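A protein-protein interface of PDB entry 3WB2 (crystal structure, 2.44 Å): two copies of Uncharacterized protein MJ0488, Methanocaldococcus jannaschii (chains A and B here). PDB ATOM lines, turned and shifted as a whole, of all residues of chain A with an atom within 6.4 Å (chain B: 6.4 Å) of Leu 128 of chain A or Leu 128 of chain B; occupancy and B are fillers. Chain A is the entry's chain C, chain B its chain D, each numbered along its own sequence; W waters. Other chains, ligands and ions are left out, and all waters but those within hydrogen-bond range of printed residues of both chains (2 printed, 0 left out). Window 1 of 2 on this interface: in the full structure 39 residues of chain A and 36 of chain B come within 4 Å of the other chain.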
ATOM      1  N   LEU A 105      35.583 -17.997 -11.925  1.00  0.00           N
ATOM      2  CA  LEU A 105      35.961 -17.287 -13.163  1.00  0.00           C
ATOM      3  C   LEU A 105      37.481 -17.368 -13.459  1.00  0.00           C
ATOM      4  O   LEU A 105      37.870 -17.942 -14.497  1.00  0.00           O
ATOM      5  CB  LEU A 105      35.488 -15.834 -13.053  1.00  0.00           C
ATOM      6  CG  LEU A 105      36.113 -14.748 -13.928  1.00  0.00           C
ATOM      7  CD1 LEU A 105      35.709 -14.981 -15.386  1.00  0.00           C
ATOM      8  CD2 LEU A 105      35.792 -13.289 -13.536  1.00  0.00           C
ATOM      9  N   SER A 112      32.300 -16.060  -9.494  1.00  0.00           N
ATOM     10  CA  SER A 112      31.788 -17.143 -10.313  1.00  0.00           C
ATOM     11  C   SER A 112      31.523 -16.910 -11.756  1.00  0.00           C
ATOM     12  O   SER A 112      31.252 -15.807 -12.203  1.00  0.00           O
ATOM     13  CB  SER A 112      30.468 -17.588  -9.749  1.00  0.00           C
ATOM     14  OG  SER A 112      30.730 -18.251  -8.518  1.00  0.00           O
ATOM     15  N   MET A 113      31.560 -18.013 -12.487  1.00  0.00           N
ATOM     16  CA  MET A 113      31.177 -18.061 -13.895  1.00  0.00           C
ATOM     17  C   MET A 113      30.394 -19.350 -14.175  1.00  0.00           C
ATOM     18  O   MET A 113      30.844 -20.452 -13.829  1.00  0.00           O
ATOM     19  CB  MET A 113      32.419 -17.974 -14.824  1.00  0.00           C
ATOM     20  CG  MET A 113      32.157 -18.407 -16.271  1.00  0.00           C
ATOM     21  SD  MET A 113      33.488 -18.251 -17.528  1.00  0.00           S
ATOM     22  CE  MET A 113      33.099 -16.653 -18.211  1.00  0.00           C
ATOM     23  N   LEU A 114      29.233 -19.188 -14.791  1.00  0.00           N
ATOM     24  CA  LEU A 114      28.519 -20.268 -15.433  1.00  0.00           C
ATOM     25  C   LEU A 114      28.616 -20.067 -16.961  1.00  0.00           C
ATOM     26  O   LEU A 114      28.284 -18.984 -17.491  1.00  0.00           O
ATOM     27  CB  LEU A 114      27.058 -20.276 -15.006  1.00  0.00           C
ATOM     28  CG  LEU A 114      26.149 -21.428 -15.471  1.00  0.00           C
ATOM     29  CD1 LEU A 114      25.271 -21.883 -14.308  1.00  0.00           C
ATOM     30  CD2 LEU A 114      25.325 -21.066 -16.678  1.00  0.00           C
ATOM     31  N   THR A 125      27.329 -18.712 -24.387  1.00  0.00           N
ATOM     32  CA  THR A 125      26.799 -17.717 -23.445  1.00  0.00           C
ATOM     33  C   THR A 125      27.396 -17.999 -22.039  1.00  0.00           C
ATOM     34  O   THR A 125      27.912 -19.098 -21.802  1.00  0.00           O
ATOM     35  CB  THR A 125      25.245 -17.767 -23.376  1.00  0.00           C
ATOM     36  OG1 THR A 125      24.745 -16.691 -22.567  1.00  0.00           O
ATOM     37  CG2 THR A 125      24.788 -19.049 -22.755  1.00  0.00           C
ATOM     38  N   ALA A 126      27.315 -17.022 -21.136  1.00  0.00           N
ATOM     39  CA  ALA A 126      27.841 -17.123 -19.761  1.00  0.00           C
ATOM     40  C   ALA A 126      27.236 -16.039 -18.820  1.00  0.00           C
ATOM     41  O   ALA A 126      26.716 -15.050 -19.303  1.00  0.00           O
ATOM     42  CB  ALA A 126      29.354 -16.967 -19.788  1.00  0.00           C
ATOM     43  N   SER A 127      27.319 -16.222 -17.495  1.00  0.00           N
ATOM     44  CA  SER A 127      26.944 -15.174 -16.524  1.00  0.00           C
ATOM     45  C   SER A 127      27.844 -15.251 -15.309  1.00  0.00           C
ATOM     46  O   SER A 127      28.392 -16.310 -15.039  1.00  0.00           O
ATOM     47  CB  SER A 127      25.483 -15.309 -16.118  1.00  0.00           C
ATOM     48  OG  SER A 127      25.260 -16.657 -15.776  1.00  0.00           O
ATOM     49  N   LEU A 128      28.011 -14.139 -14.588  1.00  0.00           N
ATOM     50  CA  LEU A 128      29.009 -14.008 -13.480  1.00  0.00           C
ATOM     51  C   LEU A 128      28.377 -13.560 -12.143  1.00  0.00           C
ATOM     52  O   LEU A 128      27.480 -12.739 -12.155  1.00  0.00           O
ATOM     53  CB  LEU A 128      30.126 -13.013 -13.855  1.00  0.00           C
ATOM     54  CG  LEU A 128      30.779 -13.098 -15.241  1.00  0.00           C
ATOM     55  CD1 LEU A 128      31.628 -11.861 -15.534  1.00  0.00           C
ATOM     56  CD2 LEU A 128      31.609 -14.365 -15.407  1.00  0.00           C
ATOM     57  N   SER A 129      28.853 -14.065 -10.999  1.00  0.00           N
ATOM     58  CA  SER A 129      28.484 -13.484  -9.690  1.00  0.00           C
ATOM     59  C   SER A 129      29.737 -13.098  -8.931  1.00  0.00           C
ATOM     60  O   SER A 129      30.816 -13.637  -9.208  1.00  0.00           O
ATOM     61  CB  SER A 129      27.691 -14.465  -8.816  1.00  0.00           C
ATOM     62  OG  SER A 129      26.549 -14.975  -9.477  1.00  0.00           O
ATOM     63  N   PRO A 130      29.611 -12.136  -7.990  1.00  0.00           N
ATOM     64  CA  PRO A 130      30.722 -11.845  -7.040  1.00  0.00           C
ATOM     65  C   PRO A 130      31.021 -13.037  -6.094  1.00  0.00           C
ATOM     66  O   PRO A 130      30.297 -14.044  -6.126  1.00  0.00           O
ATOM     67  CB  PRO A 130      30.200 -10.672  -6.212  1.00  0.00           C
ATOM     68  CG  PRO A 130      28.884 -10.274  -6.808  1.00  0.00           C
ATOM     69  CD  PRO A 130      28.440 -11.250  -7.827  1.00  0.00           C
ATOM     70  N   ARG A 142      21.906 -18.765  -6.191  1.00  0.00           N
ATOM     71  CA  ARG A 142      22.852 -18.138  -7.065  1.00  0.00           C
ATOM     72  C   ARG A 142      22.958 -18.819  -8.426  1.00  0.00           C
ATOM     73  O   ARG A 142      22.998 -18.133  -9.464  1.00  0.00           O
ATOM     74  CB  ARG A 142      24.208 -18.152  -6.379  1.00  0.00           C
ATOM     75  CG  ARG A 142      25.001 -16.892  -6.608  1.00  0.00           C
ATOM     76  CD  ARG A 142      24.107 -15.713  -6.326  1.00  0.00           C
ATOM     77  NE  ARG A 142      24.368 -14.685  -7.307  1.00  0.00           N
ATOM     78  CZ  ARG A 142      24.012 -13.414  -7.163  1.00  0.00           C
ATOM     79  NH1 ARG A 142      23.366 -13.012  -6.067  1.00  0.00           N
ATOM     80  NH2 ARG A 142      24.314 -12.544  -8.118  1.00  0.00           N
ATOM     81  N   GLU A 146      22.088 -17.413 -12.130  1.00  0.00           N
ATOM     82  CA  GLU A 146      23.112 -17.363 -13.171  1.00  0.00           C
ATOM     83  C   GLU A 146      22.577 -17.980 -14.459  1.00  0.00           C
ATOM     84  O   GLU A 146      22.698 -17.384 -15.545  1.00  0.00           O
ATOM     85  CB  GLU A 146      24.445 -17.982 -12.711  1.00  0.00           C
ATOM     86  CG  GLU A 146      25.137 -17.238 -11.556  1.00  0.00           C
ATOM     87  CD  GLU A 146      26.211 -18.040 -10.785  1.00  0.00           C
ATOM     88  OE1 GLU A 146      26.357 -19.282 -10.943  1.00  0.00           O
ATOM     89  OE2 GLU A 146      26.942 -17.398  -9.994  1.00  0.00           O
ATOM     90  N   GLU A 149      19.816 -15.654 -16.288  1.00  0.00           N
ATOM     91  CA  GLU A 149      20.529 -14.600 -17.055  1.00  0.00           C
ATOM     92  C   GLU A 149      21.313 -15.117 -18.313  1.00  0.00           C
ATOM     93  O   GLU A 149      21.333 -14.458 -19.361  1.00  0.00           O
ATOM     94  CB  GLU A 149      21.434 -13.684 -16.174  1.00  0.00           C
ATOM     95  CG  GLU A 149      22.087 -12.582 -17.028  1.00  0.00           C
ATOM     96  CD  GLU A 149      23.011 -11.603 -16.293  1.00  0.00           C
ATOM     97  OE1 GLU A 149      23.915 -12.042 -15.535  1.00  0.00           O
ATOM     98  OE2 GLU A 149      22.865 -10.372 -16.519  1.00  0.00           O
ATOM     99  N   ARG A 153      20.092 -13.423 -22.002  1.00  0.00           N
ATOM    100  CA  ARG A 153      21.034 -12.575 -22.729  1.00  0.00           C
ATOM    101  C   ARG A 153      21.243 -13.042 -24.177  1.00  0.00           C
ATOM    102  O   ARG A 153      21.723 -12.265 -25.012  1.00  0.00           O
ATOM    103  CB  ARG A 153      22.369 -12.466 -21.980  1.00  0.00           C
ATOM    104  CG  ARG A 153      23.291 -13.682 -22.086  1.00  0.00           C
ATOM    105  CD  ARG A 153      24.430 -13.528 -21.052  1.00  0.00           C
ATOM    106  NE  ARG A 153      25.416 -12.573 -21.504  1.00  0.00           N
ATOM    107  CZ  ARG A 153      26.246 -12.831 -22.498  1.00  0.00           C
ATOM    108  NH1 ARG A 153      27.118 -11.928 -22.917  1.00  0.00           N
ATOM    109  NH2 ARG A 153      26.216 -14.004 -23.083  1.00  0.00           N
ATOM    110  N   LEU B 105      32.698 -11.920 -26.333  1.00  0.00           N
ATOM    111  CA  LEU B 105      32.939 -12.916 -25.302  1.00  0.00           C
ATOM    112  C   LEU B 105      33.499 -14.239 -25.859  1.00  0.00           C
ATOM    113  O   LEU B 105      34.592 -14.693 -25.436  1.00  0.00           O
ATOM    114  CB  LEU B 105      31.625 -13.153 -24.535  1.00  0.00           C
ATOM    115  CG  LEU B 105      31.575 -14.431 -23.691  1.00  0.00           C
ATOM    116  CD1 LEU B 105      32.596 -14.374 -22.556  1.00  0.00           C
ATOM    117  CD2 LEU B 105      30.174 -14.720 -23.148  1.00  0.00           C
ATOM    118  N   SER B 112      29.088  -9.431 -25.328  1.00  0.00           N
ATOM    119  CA  SER B 112      30.312  -8.747 -24.880  1.00  0.00           C
ATOM    120  C   SER B 112      30.934  -9.239 -23.587  1.00  0.00           C
ATOM    121  O   SER B 112      30.221  -9.656 -22.671  1.00  0.00           O
ATOM    122  CB  SER B 112      29.996  -7.286 -24.636  1.00  0.00           C
ATOM    123  OG  SER B 112      30.307  -6.578 -25.799  1.00  0.00           O
ATOM    124  N   MET B 113      32.265  -9.093 -23.486  1.00  0.00           N
ATOM    125  CA  MET B 113      32.966  -9.182 -22.205  1.00  0.00           C
ATOM    126  C   MET B 113      33.950  -7.994 -21.970  1.00  0.00           C
ATOM    127  O   MET B 113      34.654  -7.589 -22.899  1.00  0.00           O
ATOM    128  CB  MET B 113      33.685 -10.529 -22.130  1.00  0.00           C
ATOM    129  CG  MET B 113      34.551 -10.716 -20.881  1.00  0.00           C
ATOM    130  SD  MET B 113      35.547 -12.236 -20.939  1.00  0.00           S
ATOM    131  CE  MET B 113      34.817 -13.217 -19.655  1.00  0.00           C
ATOM    132  N   LEU B 114      33.997  -7.432 -20.760  1.00  0.00           N
ATOM    133  CA  LEU B 114      35.096  -6.532 -20.377  1.00  0.00           C
ATOM    134  C   LEU B 114      35.853  -7.254 -19.314  1.00  0.00           C
ATOM    135  O   LEU B 114      35.219  -7.729 -18.389  1.00  0.00           O
ATOM    136  CB  LEU B 114      34.585  -5.233 -19.764  1.00  0.00           C
ATOM    137  CG  LEU B 114      35.577  -4.157 -19.227  1.00  0.00           C
ATOM    138  CD1 LEU B 114      35.050  -2.724 -19.366  1.00  0.00           C
ATOM    139  CD2 LEU B 114      35.955  -4.423 -17.785  1.00  0.00           C
ATOM    140  N   THR B 125      39.004  -9.812 -12.634  1.00  0.00           N
ATOM    141  CA  THR B 125      37.561  -9.498 -12.660  1.00  0.00           C
ATOM    142  C   THR B 125      37.033  -9.314 -14.096  1.00  0.00           C
ATOM    143  O   THR B 125      37.821  -9.156 -15.026  1.00  0.00           O
ATOM    144  CB  THR B 125      37.221  -8.285 -11.759  1.00  0.00           C
ATOM    145  OG1 THR B 125      35.804  -8.171 -11.679  1.00  0.00           O
ATOM    146  CG2 THR B 125      37.815  -6.968 -12.289  1.00  0.00           C
ATOM    147  N   ALA B 126      35.715  -9.368 -14.287  1.00  0.00           N
ATOM    148  CA  ALA B 126      35.131  -9.215 -15.657  1.00  0.00           C
ATOM    149  C   ALA B 126      33.630  -8.862 -15.613  1.00  0.00           C
ATOM    150  O   ALA B 126      33.007  -8.969 -14.574  1.00  0.00           O
ATOM    151  CB  ALA B 126      35.363 -10.466 -16.497  1.00  0.00           C
ATOM    152  N   SER B 127      33.049  -8.491 -16.748  1.00  0.00           N
ATOM    153  CA  SER B 127      31.660  -8.086 -16.799  1.00  0.00           C
ATOM    154  C   SER B 127      31.052  -8.394 -18.175  1.00  0.00           C
ATOM    155  O   SER B 127      31.762  -8.427 -19.149  1.00  0.00           O
ATOM    156  CB  SER B 127      31.615  -6.598 -16.538  1.00  0.00           C
ATOM    157  OG  SER B 127      30.343  -6.234 -16.112  1.00  0.00           O
ATOM    158  N   LEU B 128      29.739  -8.610 -18.261  1.00  0.00           N
ATOM    159  CA  LEU B 128      29.151  -9.083 -19.504  1.00  0.00           C
ATOM    160  C   LEU B 128      27.936  -8.287 -19.936  1.00  0.00           C
ATOM    161  O   LEU B 128      27.186  -7.807 -19.084  1.00  0.00           O
ATOM    162  CB  LEU B 128      28.749 -10.549 -19.374  1.00  0.00           C
ATOM    163  CG  LEU B 128      29.740 -11.639 -18.997  1.00  0.00           C
ATOM    164  CD1 LEU B 128      29.032 -12.944 -19.295  1.00  0.00           C
ATOM    165  CD2 LEU B 128      31.089 -11.609 -19.731  1.00  0.00           C
ATOM    166  N   SER B 129      27.729  -8.199 -21.254  1.00  0.00           N
ATOM    167  CA  SER B 129      26.514  -7.574 -21.854  1.00  0.00           C
ATOM    168  C   SER B 129      25.889  -8.450 -22.929  1.00  0.00           C
ATOM    169  O   SER B 129      26.616  -9.211 -23.585  1.00  0.00           O
ATOM    170  CB  SER B 129      26.857  -6.246 -22.516  1.00  0.00           C
ATOM    171  OG  SER B 129      27.028  -5.233 -21.557  1.00  0.00           O
ATOM    172  N   PRO B 130      24.551  -8.358 -23.114  1.00  0.00           N
ATOM    173  CA  PRO B 130      23.927  -9.062 -24.240  1.00  0.00           C
ATOM    174  C   PRO B 130      24.377  -8.460 -25.579  1.00  0.00           C
ATOM    175  O   PRO B 130      24.983  -7.381 -25.594  1.00  0.00           O
ATOM    176  CB  PRO B 130      22.406  -8.819 -24.009  1.00  0.00           C
ATOM    177  CG  PRO B 130      22.260  -8.512 -22.540  1.00  0.00           C
ATOM    178  CD  PRO B 130      23.535  -7.778 -22.201  1.00  0.00           C
ATOM    179  N   ARG B 142      27.261   1.334 -22.449  1.00  0.00           N
ATOM    180  CA  ARG B 142      27.412  -0.063 -22.073  1.00  0.00           C
ATOM    181  C   ARG B 142      28.765  -0.255 -21.342  1.00  0.00           C
ATOM    182  O   ARG B 142      28.832  -0.880 -20.262  1.00  0.00           O
ATOM    183  CB  ARG B 142      27.301  -0.955 -23.315  1.00  0.00           C
ATOM    184  CG  ARG B 142      26.436  -2.197 -23.132  1.00  0.00           C
ATOM    185  CD  ARG B 142      25.069  -1.823 -22.559  1.00  0.00           C
ATOM    186  NE  ARG B 142      24.287  -2.955 -22.044  1.00  0.00           N
ATOM    187  CZ  ARG B 142      24.502  -3.593 -20.886  1.00  0.00           C
ATOM    188  NH1 ARG B 142      25.514  -3.258 -20.096  1.00  0.00           N
ATOM    189  NH2 ARG B 142      23.713  -4.601 -20.532  1.00  0.00           N
ATOM    190  N   GLU B 146      29.513  -1.942 -17.643  1.00  0.00           N
ATOM    191  CA  GLU B 146      30.343  -3.134 -17.528  1.00  0.00           C
ATOM    192  C   GLU B 146      31.539  -2.852 -16.586  1.00  0.00           C
ATOM    193  O   GLU B 146      31.850  -3.659 -15.706  1.00  0.00           O
ATOM    194  CB  GLU B 146      30.816  -3.635 -18.906  1.00  0.00           C
ATOM    195  CG  GLU B 146      29.721  -4.179 -19.837  1.00  0.00           C
ATOM    196  CD  GLU B 146      30.129  -4.153 -21.318  1.00  0.00           C
ATOM    197  OE1 GLU B 146      31.315  -3.951 -21.648  1.00  0.00           O
ATOM    198  OE2 GLU B 146      29.270  -4.368 -22.199  1.00  0.00           O
ATOM    199  N   GLU B 149      30.293  -2.403 -12.668  1.00  0.00           N
ATOM    200  CA  GLU B 149      30.021  -3.727 -12.116  1.00  0.00           C
ATOM    201  C   GLU B 149      31.313  -4.606 -11.952  1.00  0.00           C
ATOM    202  O   GLU B 149      31.425  -5.358 -10.999  1.00  0.00           O
ATOM    203  CB  GLU B 149      28.905  -4.425 -12.914  1.00  0.00           C
ATOM    204  CG  GLU B 149      28.999  -5.944 -12.982  1.00  0.00           C
ATOM    205  CD  GLU B 149      27.705  -6.604 -13.465  1.00  0.00           C
ATOM    206  OE1 GLU B 149      27.479  -6.747 -14.704  1.00  0.00           O
ATOM    207  OE2 GLU B 149      26.903  -6.998 -12.588  1.00  0.00           O
ATOM    208  N   ARG B 153      31.851  -5.909  -7.973  1.00  0.00           N
ATOM    209  CA  ARG B 153      31.858  -7.365  -7.662  1.00  0.00           C
ATOM    210  C   ARG B 153      33.134  -7.891  -6.963  1.00  0.00           C
ATOM    211  O   ARG B 153      33.132  -8.971  -6.388  1.00  0.00           O
ATOM    212  CB  ARG B 153      31.574  -8.196  -8.932  1.00  0.00           C
ATOM    213  CG  ARG B 153      32.693  -8.160  -9.965  1.00  0.00           C
ATOM    214  CD  ARG B 153      32.269  -8.806 -11.265  1.00  0.00           C
ATOM    215  NE  ARG B 153      32.060 -10.249 -11.125  1.00  0.00           N
ATOM    216  CZ  ARG B 153      33.045 -11.141 -11.054  1.00  0.00           C
ATOM    217  NH1 ARG B 153      32.771 -12.453 -10.952  1.00  0.00           N
ATOM    218  NH2 ARG B 153      34.309 -10.722 -11.094  1.00  0.00           N
HETATM  219  O   HOH W   1      25.031 -10.208 -19.974  1.00  0.00           O
HETATM  220  O   HOH W   2      28.955 -10.541 -11.129  1.00  0.00           O
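Leu 105 of chain A touches Arg 153 of chain B, but with the chains exchanged Arg 153 of chain A does not touch Leu 105 of chain B (4.02 Å).
Ser 112 of chain A touches Arg 153 of chain B, and with the chains exchanged Arg 153 of chain A touches Ser 112 of chain B.
Leu 128 of chain A touches Ser 127 of chain B, but with the chains exchanged Ser 127 of chain A does not touch Leu 128 of chain B (4.1 Å).
Ser 129 of chain A touches Arg 153 of chain B, and with the chains exchanged Arg 153 of chain A touches Ser 129 of chain B.
Of the 13 pairs that touch across the chains among the printed residues, 9 have their exchanged pair printed and touching as well.
The backbone carbonyl oxygen of Ser 129 of chain A sits at hydrogen-bond distance from the backbone NH of Ser 112 of chain A (2.9 Å).
The side-chain hydroxyl (OG1) of Thr 125 of chain A is in hydrogen-bond range of the guanidinium group (NH2) of Arg 153 of chain A.
The backbone carbonyl oxygen (O) of Leu 114 of chain B is in hydrogen-bond range of the backbone NH (N) of Ser 127 of chain B (2.8 Å).
O of Glu 146 of chain B sits at hydrogen-bond distance from OG of Ser 127 of chain B, at 3.0 Å.
The side-chain hydroxyl (OG) of Ser 129 of chain B lies within hydrogen-bond range of the guanidinium group (NH1) of Arg 142 of chain B (2.9 Å).
OE2 of Glu 146 of chain B lies within hydrogen-bond range of OG of Ser 129 of chain B (2.5 Å).
NH1 of Arg 153 of chain B lies within hydrogen-bond range of O of Ser 129 of chain A (2.9 Å).
The backbone carbonyl oxygen (O) of Ser 129 of chain B lies within hydrogen-bond range of the guanidinium group (NH1) of Arg 153 of chain A (2.8 Å).
Water W2 lies within hydrogen-bond range of O of Leu 128 of chain A and NE of Arg 153 of chain B.
Water W1 lies within hydrogen-bond range of NE of Arg 153 of chain A (2.8 Å) and O of Leu 128 of chain B (3.3 Å).
Leu 105 of chain A touches Ala 126 of chain B (CD2 to N, 3.99 Å).
CD2 of Leu 105 of chain A touches NH2 of Arg 153 of chain B, at 3.8 Å.
Ser 112 of chain A touches Arg 153 of chain B.
Ala 126 of chain A touches Leu 128 of chain B.
O of Ala 126 of chain B touches CD1 of Leu 128 of chain A (3.3 Å).
CD1 of Leu 128 of chain A touches N of Ser 127 of chain B (3.9 Å).
Leu 128 of chain B touches Leu 128 of chain A.
Arg 153 of chain B touches Leu 128 of chain A.
Pro 130 of chain A touches Arg 153 of chain B (CB to O, 3.4 Å).
Arg 153 of chain A touches Pro 130 of chain B (O to CB, 3.7 Å).
Thr 125 of chain B touches none of the printed residues of chain A.
Of chain A, only Ala 126 and Leu 128 come within 4 Å of Leu 128 of chain B.
Printed residues of chain A within 4 Å of Ser 129 of chain B: Arg 153 (2.8 Å).
Printed residues of chain A within 4 Å of Arg 153 of chain B: Leu 105, Ser 112, Leu 128, Ser 129 and Pro 130.
The nearest residue of chain B that does not touch Leu 128 of chain A is Met 113 of chain B (5.4 Å).
The nearest printed residue of chain A that does not touch Leu 128 of chain B is Ser 127 of chain A (4.1 Å).
Of the 14 printed residues of chain A, 7 touch a printed residue of chain B.
Printed residues of chain A that touch a printed residue of chain B: Leu 105, Ser 112, Ala 126, Leu 128, Ser 129, Pro 130 and Arg 153.
Hydrophobic or aromatic side chains of chain A that line the printed part of chain B: Leu 105, Leu 128 and Pro 130.
Along chain A the printed residues that touch a printed residue of chain B span positions 105 to 153.
Hydrophobic or aromatic side chains of chain B within 4 Å of the printed part of chain A: Leu 128 and Pro 130.
Among the printed residues, no Asp or Glu carboxylate lies within 4 Å of a Lys or Arg side-chain nitrogen of the other chain.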
